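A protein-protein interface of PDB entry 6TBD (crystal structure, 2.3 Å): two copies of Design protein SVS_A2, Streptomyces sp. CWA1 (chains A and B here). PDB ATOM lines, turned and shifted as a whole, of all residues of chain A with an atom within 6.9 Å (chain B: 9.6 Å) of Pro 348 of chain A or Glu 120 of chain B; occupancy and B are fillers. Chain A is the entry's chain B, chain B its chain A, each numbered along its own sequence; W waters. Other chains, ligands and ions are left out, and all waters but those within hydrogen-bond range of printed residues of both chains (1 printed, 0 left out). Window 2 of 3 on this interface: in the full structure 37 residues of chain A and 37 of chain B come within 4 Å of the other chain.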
ATOM      1  N   LEU A 175     -23.017  -2.479  22.622  1.00  0.00           N
ATOM      2  CA  LEU A 175     -24.164  -2.543  21.756  1.00  0.00           C
ATOM      3  C   LEU A 175     -23.769  -2.198  20.292  1.00  0.00           C
ATOM      4  O   LEU A 175     -24.210  -2.881  19.373  1.00  0.00           O
ATOM      5  CB  LEU A 175     -25.251  -1.600  22.294  1.00  0.00           C
ATOM      6  CG  LEU A 175     -26.532  -1.467  21.474  1.00  0.00           C
ATOM      7  CD1 LEU A 175     -27.228  -2.819  21.372  1.00  0.00           C
ATOM      8  CD2 LEU A 175     -27.476  -0.460  22.098  1.00  0.00           C
ATOM      9  N   ASP A 176     -22.939  -1.175  20.097  1.00  0.00           N
ATOM     10  CA  ASP A 176     -22.557  -0.723  18.763  1.00  0.00           C
ATOM     11  C   ASP A 176     -21.789  -1.802  17.976  1.00  0.00           C
ATOM     12  O   ASP A 176     -22.191  -2.186  16.885  1.00  0.00           O
ATOM     13  CB  ASP A 176     -21.720   0.548  18.801  1.00  0.00           C
ATOM     14  CG  ASP A 176     -21.626   1.244  17.417  1.00  0.00           C
ATOM     15  OD1 ASP A 176     -22.662   1.474  16.759  1.00  0.00           O
ATOM     16  OD2 ASP A 176     -20.514   1.548  16.960  1.00  0.00           O
ATOM     17  N   LEU A 344     -31.187   4.622  17.552  1.00  0.00           N
ATOM     18  CA  LEU A 344     -30.748   4.038  18.780  1.00  0.00           C
ATOM     19  C   LEU A 344     -29.551   4.810  19.368  1.00  0.00           C
ATOM     20  O   LEU A 344     -28.497   4.937  18.723  1.00  0.00           O
ATOM     21  CB  LEU A 344     -30.341   2.593  18.574  1.00  0.00           C
ATOM     22  CG  LEU A 344     -31.465   1.636  18.234  1.00  0.00           C
ATOM     23  CD1 LEU A 344     -30.904   0.227  18.249  1.00  0.00           C
ATOM     24  CD2 LEU A 344     -32.620   1.767  19.232  1.00  0.00           C
ATOM     25  N   PRO A 345     -29.722   5.361  20.582  1.00  0.00           N
ATOM     26  CA  PRO A 345     -28.539   5.890  21.258  1.00  0.00           C
ATOM     27  C   PRO A 345     -27.645   4.717  21.662  1.00  0.00           C
ATOM     28  O   PRO A 345     -28.142   3.633  22.016  1.00  0.00           O
ATOM     29  CB  PRO A 345     -29.120   6.642  22.474  1.00  0.00           C
ATOM     30  CG  PRO A 345     -30.398   5.925  22.762  1.00  0.00           C
ATOM     31  CD  PRO A 345     -30.931   5.426  21.433  1.00  0.00           C
ATOM     32  N   GLY A 346     -26.336   4.927  21.577  1.00  0.00           N
ATOM     33  CA  GLY A 346     -25.392   3.870  21.904  1.00  0.00           C
ATOM     34  C   GLY A 346     -25.106   2.938  20.735  1.00  0.00           C
ATOM     35  O   GLY A 346     -24.330   1.974  20.904  1.00  0.00           O
ATOM     36  N   ALA A 347     -25.675   3.248  19.546  1.00  0.00           N
ATOM     37  CA  ALA A 347     -25.404   2.489  18.321  1.00  0.00           C
ATOM     38  C   ALA A 347     -25.124   3.401  17.133  1.00  0.00           C
ATOM     39  O   ALA A 347     -25.829   3.382  16.155  1.00  0.00           O
ATOM     40  CB  ALA A 347     -26.554   1.546  18.053  1.00  0.00           C
ATOM     41  N   PRO A 348     -24.054   4.185  17.206  1.00  0.00           N
ATOM     42  CA  PRO A 348     -23.726   5.102  16.117  1.00  0.00           C
ATOM     43  C   PRO A 348     -23.477   4.486  14.722  1.00  0.00           C
ATOM     44  O   PRO A 348     -23.706   5.159  13.724  1.00  0.00           O
ATOM     45  CB  PRO A 348     -22.501   5.831  16.649  1.00  0.00           C
ATOM     46  CG  PRO A 348     -21.929   4.914  17.685  1.00  0.00           C
ATOM     47  CD  PRO A 348     -23.112   4.312  18.334  1.00  0.00           C
ATOM     48  N   SER A 349     -23.109   3.218  14.623  1.00  0.00           N
ATOM     49  CA  SER A 349     -22.861   2.609  13.292  1.00  0.00           C
ATOM     50  C   SER A 349     -24.107   2.375  12.443  1.00  0.00           C
ATOM     51  O   SER A 349     -23.989   2.159  11.265  1.00  0.00           O
ATOM     52  CB  SER A 349     -22.102   1.284  13.410  1.00  0.00           C
ATOM     53  OG  SER A 349     -22.966   0.221  13.811  1.00  0.00           O
ATOM     54  N   ILE A 350     -25.282   2.327  13.060  1.00  0.00           N
ATOM     55  CA  ILE A 350     -26.530   2.153  12.332  1.00  0.00           C
ATOM     56  C   ILE A 350     -27.353   3.432  12.343  1.00  0.00           C
ATOM     57  O   ILE A 350     -28.444   3.443  11.801  1.00  0.00           O
ATOM     58  CB  ILE A 350     -27.383   1.014  12.902  1.00  0.00           C
ATOM     59  CG1 ILE A 350     -27.899   1.377  14.292  1.00  0.00           C
ATOM     60  CG2 ILE A 350     -26.590  -0.298  12.916  1.00  0.00           C
ATOM     61  CD1 ILE A 350     -28.897   0.444  14.848  1.00  0.00           C
ATOM     62  N   ALA A 351     -26.847   4.508  12.945  1.00  0.00           N
ATOM     63  CA  ALA A 351     -27.594   5.745  13.068  1.00  0.00           C
ATOM     64  C   ALA A 351     -27.910   6.299  11.702  1.00  0.00           C
ATOM     65  O   ALA A 351     -28.977   6.914  11.522  1.00  0.00           O
ATOM     66  CB  ALA A 351     -26.846   6.769  13.893  1.00  0.00           C
ATOM     67  N   TRP A 352     -27.033   6.042  10.723  1.00  0.00           N
ATOM     68  CA  TRP A 352     -27.264   6.526   9.368  1.00  0.00           C
ATOM     69  C   TRP A 352     -28.537   5.982   8.746  1.00  0.00           C
ATOM     70  O   TRP A 352     -29.093   6.599   7.854  1.00  0.00           O
ATOM     71  CB  TRP A 352     -26.053   6.290   8.485  1.00  0.00           C
ATOM     72  CG  TRP A 352     -25.788   4.867   8.127  1.00  0.00           C
ATOM     73  CD1 TRP A 352     -25.115   3.970   8.862  1.00  0.00           C
ATOM     74  CD2 TRP A 352     -26.171   4.188   6.931  1.00  0.00           C
ATOM     75  NE1 TRP A 352     -25.029   2.778   8.215  1.00  0.00           N
ATOM     76  CE2 TRP A 352     -25.697   2.869   7.037  1.00  0.00           C
ATOM     77  CE3 TRP A 352     -26.856   4.570   5.790  1.00  0.00           C
ATOM     78  CZ2 TRP A 352     -25.870   1.931   6.062  1.00  0.00           C
ATOM     79  CZ3 TRP A 352     -27.040   3.637   4.796  1.00  0.00           C
ATOM     80  CH2 TRP A 352     -26.546   2.325   4.932  1.00  0.00           C
ATOM     81  N   LEU B 106     -10.898  -5.228  14.657  1.00  0.00           N
ATOM     82  CA  LEU B 106     -10.439  -3.956  14.033  1.00  0.00           C
ATOM     83  C   LEU B 106     -10.924  -3.865  12.573  1.00  0.00           C
ATOM     84  O   LEU B 106     -11.467  -2.883  12.146  1.00  0.00           O
ATOM     85  CB  LEU B 106      -8.931  -3.833  14.098  1.00  0.00           C
ATOM     86  CG  LEU B 106      -8.311  -2.648  13.351  1.00  0.00           C
ATOM     87  CD1 LEU B 106      -8.683  -1.334  14.002  1.00  0.00           C
ATOM     88  CD2 LEU B 106      -6.804  -2.819  13.305  1.00  0.00           C
ATOM     89  N   GLY B 108     -13.382  -5.306  11.247  1.00  0.00           N
ATOM     90  CA  GLY B 108     -14.818  -5.099  11.277  1.00  0.00           C
ATOM     91  C   GLY B 108     -15.200  -3.657  11.571  1.00  0.00           C
ATOM     92  O   GLY B 108     -16.032  -3.126  10.887  1.00  0.00           O
ATOM     93  N   ARG B 109     -14.563  -3.058  12.579  1.00  0.00           N
ATOM     94  CA  ARG B 109     -14.792  -1.669  12.957  1.00  0.00           C
ATOM     95  C   ARG B 109     -14.349  -0.750  11.814  1.00  0.00           C
ATOM     96  O   ARG B 109     -15.098   0.127  11.431  1.00  0.00           O
ATOM     97  CB  ARG B 109     -14.092  -1.285  14.287  1.00  0.00           C
ATOM     98  CG  ARG B 109     -14.619  -2.010  15.564  1.00  0.00           C
ATOM     99  CD  ARG B 109     -14.167  -1.411  16.932  1.00  0.00           C
ATOM    100  NE  ARG B 109     -12.723  -1.247  16.931  1.00  0.00           N
ATOM    101  CZ  ARG B 109     -11.817  -2.199  17.226  1.00  0.00           C
ATOM    102  NH1 ARG B 109     -12.198  -3.417  17.636  1.00  0.00           N
ATOM    103  NH2 ARG B 109     -10.500  -1.921  17.104  1.00  0.00           N
ATOM    104  N   VAL B 110     -13.131  -0.957  11.282  1.00  0.00           N
ATOM    105  CA  VAL B 110     -12.609  -0.116  10.219  1.00  0.00           C
ATOM    106  C   VAL B 110     -13.488  -0.235   8.963  1.00  0.00           C
ATOM    107  O   VAL B 110     -13.889   0.765   8.352  1.00  0.00           O
ATOM    108  CB  VAL B 110     -11.138  -0.435   9.939  1.00  0.00           C
ATOM    109  CG1 VAL B 110     -10.677   0.128   8.615  1.00  0.00           C
ATOM    110  CG2 VAL B 110     -10.293   0.133  11.044  1.00  0.00           C
ATOM    111  N   ARG B 112     -16.583  -1.092   8.847  1.00  0.00           N
ATOM    112  CA  ARG B 112     -17.921  -0.546   9.152  1.00  0.00           C
ATOM    113  C   ARG B 112     -17.869   0.985   9.012  1.00  0.00           C
ATOM    114  O   ARG B 112     -18.758   1.582   8.410  1.00  0.00           O
ATOM    115  CB  ARG B 112     -18.437  -0.983  10.531  1.00  0.00           C
ATOM    116  CG  ARG B 112     -19.852  -0.511  10.859  1.00  0.00           C
ATOM    117  CD  ARG B 112     -20.880  -1.090   9.855  1.00  0.00           C
ATOM    118  NE  ARG B 112     -22.204  -0.531   9.961  1.00  0.00           N
ATOM    119  CZ  ARG B 112     -23.174  -0.659   9.053  1.00  0.00           C
ATOM    120  NH1 ARG B 112     -23.012  -1.340   7.898  1.00  0.00           N
ATOM    121  NH2 ARG B 112     -24.369  -0.122   9.330  1.00  0.00           N
ATOM    122  N   ALA B 113     -16.810   1.595   9.528  1.00  0.00           N
ATOM    123  CA  ALA B 113     -16.582   3.045   9.400  1.00  0.00           C
ATOM    124  C   ALA B 113     -16.530   3.525   7.948  1.00  0.00           C
ATOM    125  O   ALA B 113     -16.987   4.609   7.644  1.00  0.00           O
ATOM    126  CB  ALA B 113     -15.298   3.433  10.115  1.00  0.00           C
ATOM    127  N   LEU B 114     -15.948   2.712   7.076  1.00  0.00           N
ATOM    128  CA  LEU B 114     -15.968   2.948   5.629  1.00  0.00           C
ATOM    129  C   LEU B 114     -17.376   2.942   5.043  1.00  0.00           C
ATOM    130  O   LEU B 114     -17.630   3.739   4.214  1.00  0.00           O
ATOM    131  CB  LEU B 114     -15.108   1.879   4.868  1.00  0.00           C
ATOM    132  CG  LEU B 114     -14.982   1.977   3.370  1.00  0.00           C
ATOM    133  CD1 LEU B 114     -14.507   3.362   2.933  1.00  0.00           C
ATOM    134  CD2 LEU B 114     -14.034   0.910   2.846  1.00  0.00           C
ATOM    135  N   GLU B 115     -18.253   2.039   5.490  1.00  0.00           N
ATOM    136  CA  GLU B 115     -19.635   1.896   4.977  1.00  0.00           C
ATOM    137  C   GLU B 115     -20.659   2.774   5.705  1.00  0.00           C
ATOM    138  O   GLU B 115     -21.716   3.063   5.184  1.00  0.00           O
ATOM    139  CB  GLU B 115     -20.130   0.422   5.099  1.00  0.00           C
ATOM    140  CG  GLU B 115     -19.127  -0.561   4.519  1.00  0.00           C
ATOM    141  CD  GLU B 115     -19.654  -1.926   4.150  1.00  0.00           C
ATOM    142  OE1 GLU B 115     -20.877  -2.062   4.008  1.00  0.00           O
ATOM    143  OE2 GLU B 115     -18.789  -2.860   4.002  1.00  0.00           O
ATOM    144  N   ALA B 116     -20.368   3.153   6.932  1.00  0.00           N
ATOM    145  CA  ALA B 116     -21.339   3.803   7.777  1.00  0.00           C
ATOM    146  C   ALA B 116     -20.741   5.128   8.263  1.00  0.00           C
ATOM    147  O   ALA B 116     -19.957   5.147   9.185  1.00  0.00           O
ATOM    148  CB  ALA B 116     -21.735   2.898   8.945  1.00  0.00           C
ATOM    149  N   PRO B 117     -21.112   6.246   7.628  1.00  0.00           N
ATOM    150  CA  PRO B 117     -20.592   7.576   8.005  1.00  0.00           C
ATOM    151  C   PRO B 117     -20.851   7.938   9.439  1.00  0.00           C
ATOM    152  O   PRO B 117     -20.118   8.729   9.994  1.00  0.00           O
ATOM    153  CB  PRO B 117     -21.376   8.528   7.118  1.00  0.00           C
ATOM    154  CG  PRO B 117     -21.756   7.694   5.953  1.00  0.00           C
ATOM    155  CD  PRO B 117     -22.052   6.344   6.495  1.00  0.00           C
ATOM    156  N   SER B 118     -21.872   7.339  10.044  1.00  0.00           N
ATOM    157  CA  SER B 118     -22.232   7.662  11.409  1.00  0.00           C
ATOM    158  C   SER B 118     -21.398   6.913  12.436  1.00  0.00           C
ATOM    159  O   SER B 118     -21.471   7.203  13.622  1.00  0.00           O
ATOM    160  CB  SER B 118     -23.707   7.365  11.645  1.00  0.00           C
ATOM    161  OG  SER B 118     -24.095   6.042  11.271  1.00  0.00           O
ATOM    162  N   ALA B 119     -20.595   5.958  12.002  1.00  0.00           N
ATOM    163  CA  ALA B 119     -19.706   5.268  12.893  1.00  0.00           C
ATOM    164  C   ALA B 119     -18.770   6.222  13.636  1.00  0.00           C
ATOM    165  O   ALA B 119     -18.321   7.234  13.067  1.00  0.00           O
ATOM    166  CB  ALA B 119     -18.878   4.239  12.110  1.00  0.00           C
ATOM    167  N   GLU B 120     -18.452   5.858  14.879  1.00  0.00           N
ATOM    168  CA  GLU B 120     -17.526   6.620  15.721  1.00  0.00           C
ATOM    169  C   GLU B 120     -16.170   5.958  15.814  1.00  0.00           C
ATOM    170  O   GLU B 120     -16.048   4.763  15.622  1.00  0.00           O
ATOM    171  CB  GLU B 120     -18.108   6.823  17.125  1.00  0.00           C
ATOM    172  CG  GLU B 120     -18.962   8.103  17.221  1.00  0.00           C
ATOM    173  CD  GLU B 120     -19.805   8.121  18.494  1.00  0.00           C
ATOM    174  OE1 GLU B 120     -19.407   7.415  19.469  1.00  0.00           O
ATOM    175  OE2 GLU B 120     -20.859   8.811  18.511  1.00  0.00           O
ATOM    176  N   ASP B 121     -15.148   6.752  16.102  1.00  0.00           N
ATOM    177  CA  ASP B 121     -13.768   6.285  15.935  1.00  0.00           C
ATOM    178  C   ASP B 121     -13.397   5.306  17.017  1.00  0.00           C
ATOM    179  O   ASP B 121     -12.593   4.407  16.786  1.00  0.00           O
ATOM    180  CB  ASP B 121     -12.791   7.457  15.900  1.00  0.00           C
ATOM    181  CG  ASP B 121     -12.568   8.067  17.265  1.00  0.00           C
ATOM    182  OD1 ASP B 121     -13.432   7.930  18.143  1.00  0.00           O
ATOM    183  OD2 ASP B 121     -11.507   8.654  17.490  1.00  0.00           O
ATOM    184  N   ASN B 122     -13.978   5.475  18.208  1.00  0.00           N
ATOM    185  CA  ASN B 122     -13.640   4.643  19.362  1.00  0.00           C
ATOM    186  C   ASN B 122     -12.127   4.776  19.707  1.00  0.00           C
ATOM    187  O   ASN B 122     -11.416   3.777  20.013  1.00  0.00           O
ATOM    188  CB  ASN B 122     -14.050   3.186  19.045  1.00  0.00           C
ATOM    189  CG  ASN B 122     -14.394   2.391  20.271  1.00  0.00           C
ATOM    190  OD1 ASN B 122     -13.623   1.522  20.659  1.00  0.00           O
ATOM    191  ND2 ASN B 122     -15.549   2.680  20.895  1.00  0.00           N
ATOM    192  N   GLY B 123     -11.637   6.016  19.628  1.00  0.00           N
ATOM    193  CA  GLY B 123     -10.217   6.320  19.857  1.00  0.00           C
ATOM    194  C   GLY B 123      -9.189   5.832  18.837  1.00  0.00           C
ATOM    195  O   GLY B 123      -7.979   5.993  19.061  1.00  0.00           O
ATOM    196  N   ASP B 124      -9.646   5.267  17.714  1.00  0.00           N
ATOM    197  CA  ASP B 124      -8.742   4.802  16.658  1.00  0.00           C
ATOM    198  C   ASP B 124      -8.399   5.962  15.701  1.00  0.00           C
ATOM    199  O   ASP B 124      -9.265   6.491  15.043  1.00  0.00           O
ATOM    200  CB  ASP B 124      -9.398   3.656  15.908  1.00  0.00           C
ATOM    201  CG  ASP B 124      -8.439   2.925  15.017  1.00  0.00           C
ATOM    202  OD1 ASP B 124      -7.421   3.495  14.503  1.00  0.00           O
ATOM    203  OD2 ASP B 124      -8.694   1.727  14.856  1.00  0.00           O
ATOM    204  N   ARG B 125      -7.128   6.361  15.648  1.00  0.00           N
ATOM    205  CA  ARG B 125      -6.688   7.498  14.840  1.00  0.00           C
ATOM    206  C   ARG B 125      -6.846   7.285  13.315  1.00  0.00           C
ATOM    207  O   ARG B 125      -6.926   8.251  12.531  1.00  0.00           O
ATOM    208  CB  ARG B 125      -5.230   7.832  15.172  1.00  0.00           C
ATOM    209  CG  ARG B 125      -4.187   6.743  14.875  1.00  0.00           C
ATOM    210  CD  ARG B 125      -2.885   6.997  15.627  1.00  0.00           C
ATOM    211  NE  ARG B 125      -2.038   5.795  15.774  1.00  0.00           N
ATOM    212  CZ  ARG B 125      -1.073   5.430  14.928  1.00  0.00           C
ATOM    213  NH1 ARG B 125      -0.811   6.118  13.819  1.00  0.00           N
ATOM    214  NH2 ARG B 125      -0.366   4.330  15.172  1.00  0.00           N
ATOM    215  N   PHE B 126      -6.870   6.025  12.886  1.00  0.00           N
ATOM    216  CA  PHE B 126      -7.036   5.716  11.483  1.00  0.00           C
ATOM    217  C   PHE B 126      -8.447   5.912  10.953  1.00  0.00           C
ATOM    218  O   PHE B 126      -8.609   6.089   9.736  1.00  0.00           O
ATOM    219  CB  PHE B 126      -6.538   4.316  11.159  1.00  0.00           C
ATOM    220  CG  PHE B 126      -5.059   4.226  11.115  1.00  0.00           C
ATOM    221  CD1 PHE B 126      -4.357   4.762  10.015  1.00  0.00           C
ATOM    222  CD2 PHE B 126      -4.346   3.619  12.160  1.00  0.00           C
ATOM    223  CE1 PHE B 126      -2.967   4.724   9.973  1.00  0.00           C
ATOM    224  CE2 PHE B 126      -2.958   3.585  12.126  1.00  0.00           C
ATOM    225  CZ  PHE B 126      -2.271   4.133  11.034  1.00  0.00           C
ATOM    226  N   VAL B 127      -9.443   5.883  11.839  1.00  0.00           N
ATOM    227  CA  VAL B 127     -10.858   5.844  11.421  1.00  0.00           C
ATOM    228  C   VAL B 127     -11.336   7.185  10.899  1.00  0.00           C
ATOM    229  O   VAL B 127     -11.963   7.211   9.832  1.00  0.00           O
ATOM    230  CB  VAL B 127     -11.844   5.307  12.503  1.00  0.00           C
ATOM    231  CG1 VAL B 127     -13.296   5.756  12.243  1.00  0.00           C
ATOM    232  CG2 VAL B 127     -11.755   3.800  12.557  1.00  0.00           C
ATOM    233  N   PRO B 128     -11.080   8.283  11.633  1.00  0.00           N
ATOM    234  CA  PRO B 128     -11.559   9.548  11.039  1.00  0.00           C
ATOM    235  C   PRO B 128     -10.865   9.838   9.703  1.00  0.00           C
ATOM    236  O   PRO B 128     -11.489  10.316   8.766  1.00  0.00           O
ATOM    237  CB  PRO B 128     -11.227  10.630  12.127  1.00  0.00           C
ATOM    238  CG  PRO B 128     -11.152   9.819  13.404  1.00  0.00           C
ATOM    239  CD  PRO B 128     -10.556   8.475  13.001  1.00  0.00           C
ATOM    240  N   GLN B 131     -12.652   7.808   7.167  1.00  0.00           N
ATOM    241  CA  GLN B 131     -14.015   8.312   6.958  1.00  0.00           C
ATOM    242  C   GLN B 131     -14.027   9.566   6.107  1.00  0.00           C
ATOM    243  O   GLN B 131     -15.022   9.861   5.396  1.00  0.00           O
ATOM    244  CB  GLN B 131     -14.740   8.535   8.268  1.00  0.00           C
ATOM    245  CG  GLN B 131     -15.176   7.236   8.939  1.00  0.00           C
ATOM    246  CD  GLN B 131     -16.010   7.504  10.154  1.00  0.00           C
ATOM    247  OE1 GLN B 131     -15.734   8.432  10.871  1.00  0.00           O
ATOM    248  NE2 GLN B 131     -17.070   6.712  10.365  1.00  0.00           N
HETATM  249  O   HOH W   1     -19.333   3.274  15.620  1.00  0.00           O
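Of the 11 printed residues of chain A, 4 touch a printed residue of chain B. Hydrophobic or aromatic side chains of chain A that line the printed part of chain B: Pro 348, Ala 351 and Trp 352. Of the 22 printed residues of chain B, 5 touch a printed residue of chain A. Printed residues of chain B that touch a printed residue of chain A: Arg 112, Ala 116, Ser 118, Ala 119 and Glu 120. Among the printed residues, no Asp or Glu carboxylate lies within 4 Å of a Lys or Arg side-chain nitrogen of the other chain.
Among the printed residues, pairs that only touch across the chains: Pro 348 of chain A with Ala 119 of chain B, Pro 348 of chain A with Glu 120 of chain B, Ser 349 of chain A with Ala 116 of chain B, Ser 349 of chain A with Ser 118 of chain B, Ala 351 of chain A with Ser 118 of chain B and Trp 352 of chain A with Ala 116 of chain B.
The backbone carbonyl oxygen (O) of Ala 116 of chain B lies within hydrogen-bond range of the side-chain amide nitrogen (NE2) of Gln 131 of chain B, 3.5 Å away. The side-chain carboxylate of Asp 176 of chain A is in hydrogen-bond range of the backbone NH of Ser 349 of chain A (2.8 Å). The side-chain amide nitrogen (NE2) of Gln 131 of chain B lies within hydrogen-bond range of the backbone carbonyl oxygen (O) of Ala 119 of chain B, 3.0 Å away. The backbone carbonyl oxygen of Ser 349 of chain A lies close to the indole nitrogen of Trp 352 of chain A (3.3 Å).
Pro 348 of chain A touches three residues of chain B. Glu 120 of chain B touches just one residue of chain A: Pro 348. No residue of chain B comes within 4 Å of Gly 346 of chain A. Of the printed residues of chain A, Ser 118 of chain B touches Pro 348, Ser 349, Ala 351 and Trp 352. Of the printed residues of chain B, Trp 352 of chain A touches Arg 112 (3.2 Å), Ala 116 (3.4 Å) and Ser 118 (3.0 Å). Of the printed residues of chain A, Ala 119 of chain B touches Pro 348. Printed residues of chain B within 4 Å of Ala 351 of chain A: Ser 118 (3.6 Å). Arg 109 of chain B touches none of the printed residues of chain A. Phe 126 of chain B touches none of the printed residues of chain A. The nearest printed residue of chain B that does not touch Ala 351 of chain A is Arg 112 of chain B (6.4 Å).
The side-chain hydroxyl (OG) of Ser 118 of chain B lies within hydrogen-bond range of the backbone NH (N) of Trp 352 of chain A (3.0 Å). O of Pro 348 of chain A lies within hydrogen-bond range of OG of Ser 118 of chain B, at 2.6 Å. The indole nitrogen (NE1) of Trp 352 of chain A lies close to the guanidinium group (NH2) of Arg 112 of chain B (3.2 Å). O of Ser 349 of chain A lies within hydrogen-bond range of NH2 of Arg 112 of chain B, 3.0 Å away.
Water W1 lies within hydrogen-bond range of the side-chain carboxylate (OD2) of Asp 176 of chain A and the backbone NH (N) of Glu 120 of chain B.
No position is printed for both chains. Of the 10 pairs that touch across the chains among the printed residues, none has its exchanged pair printed and touching as well.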
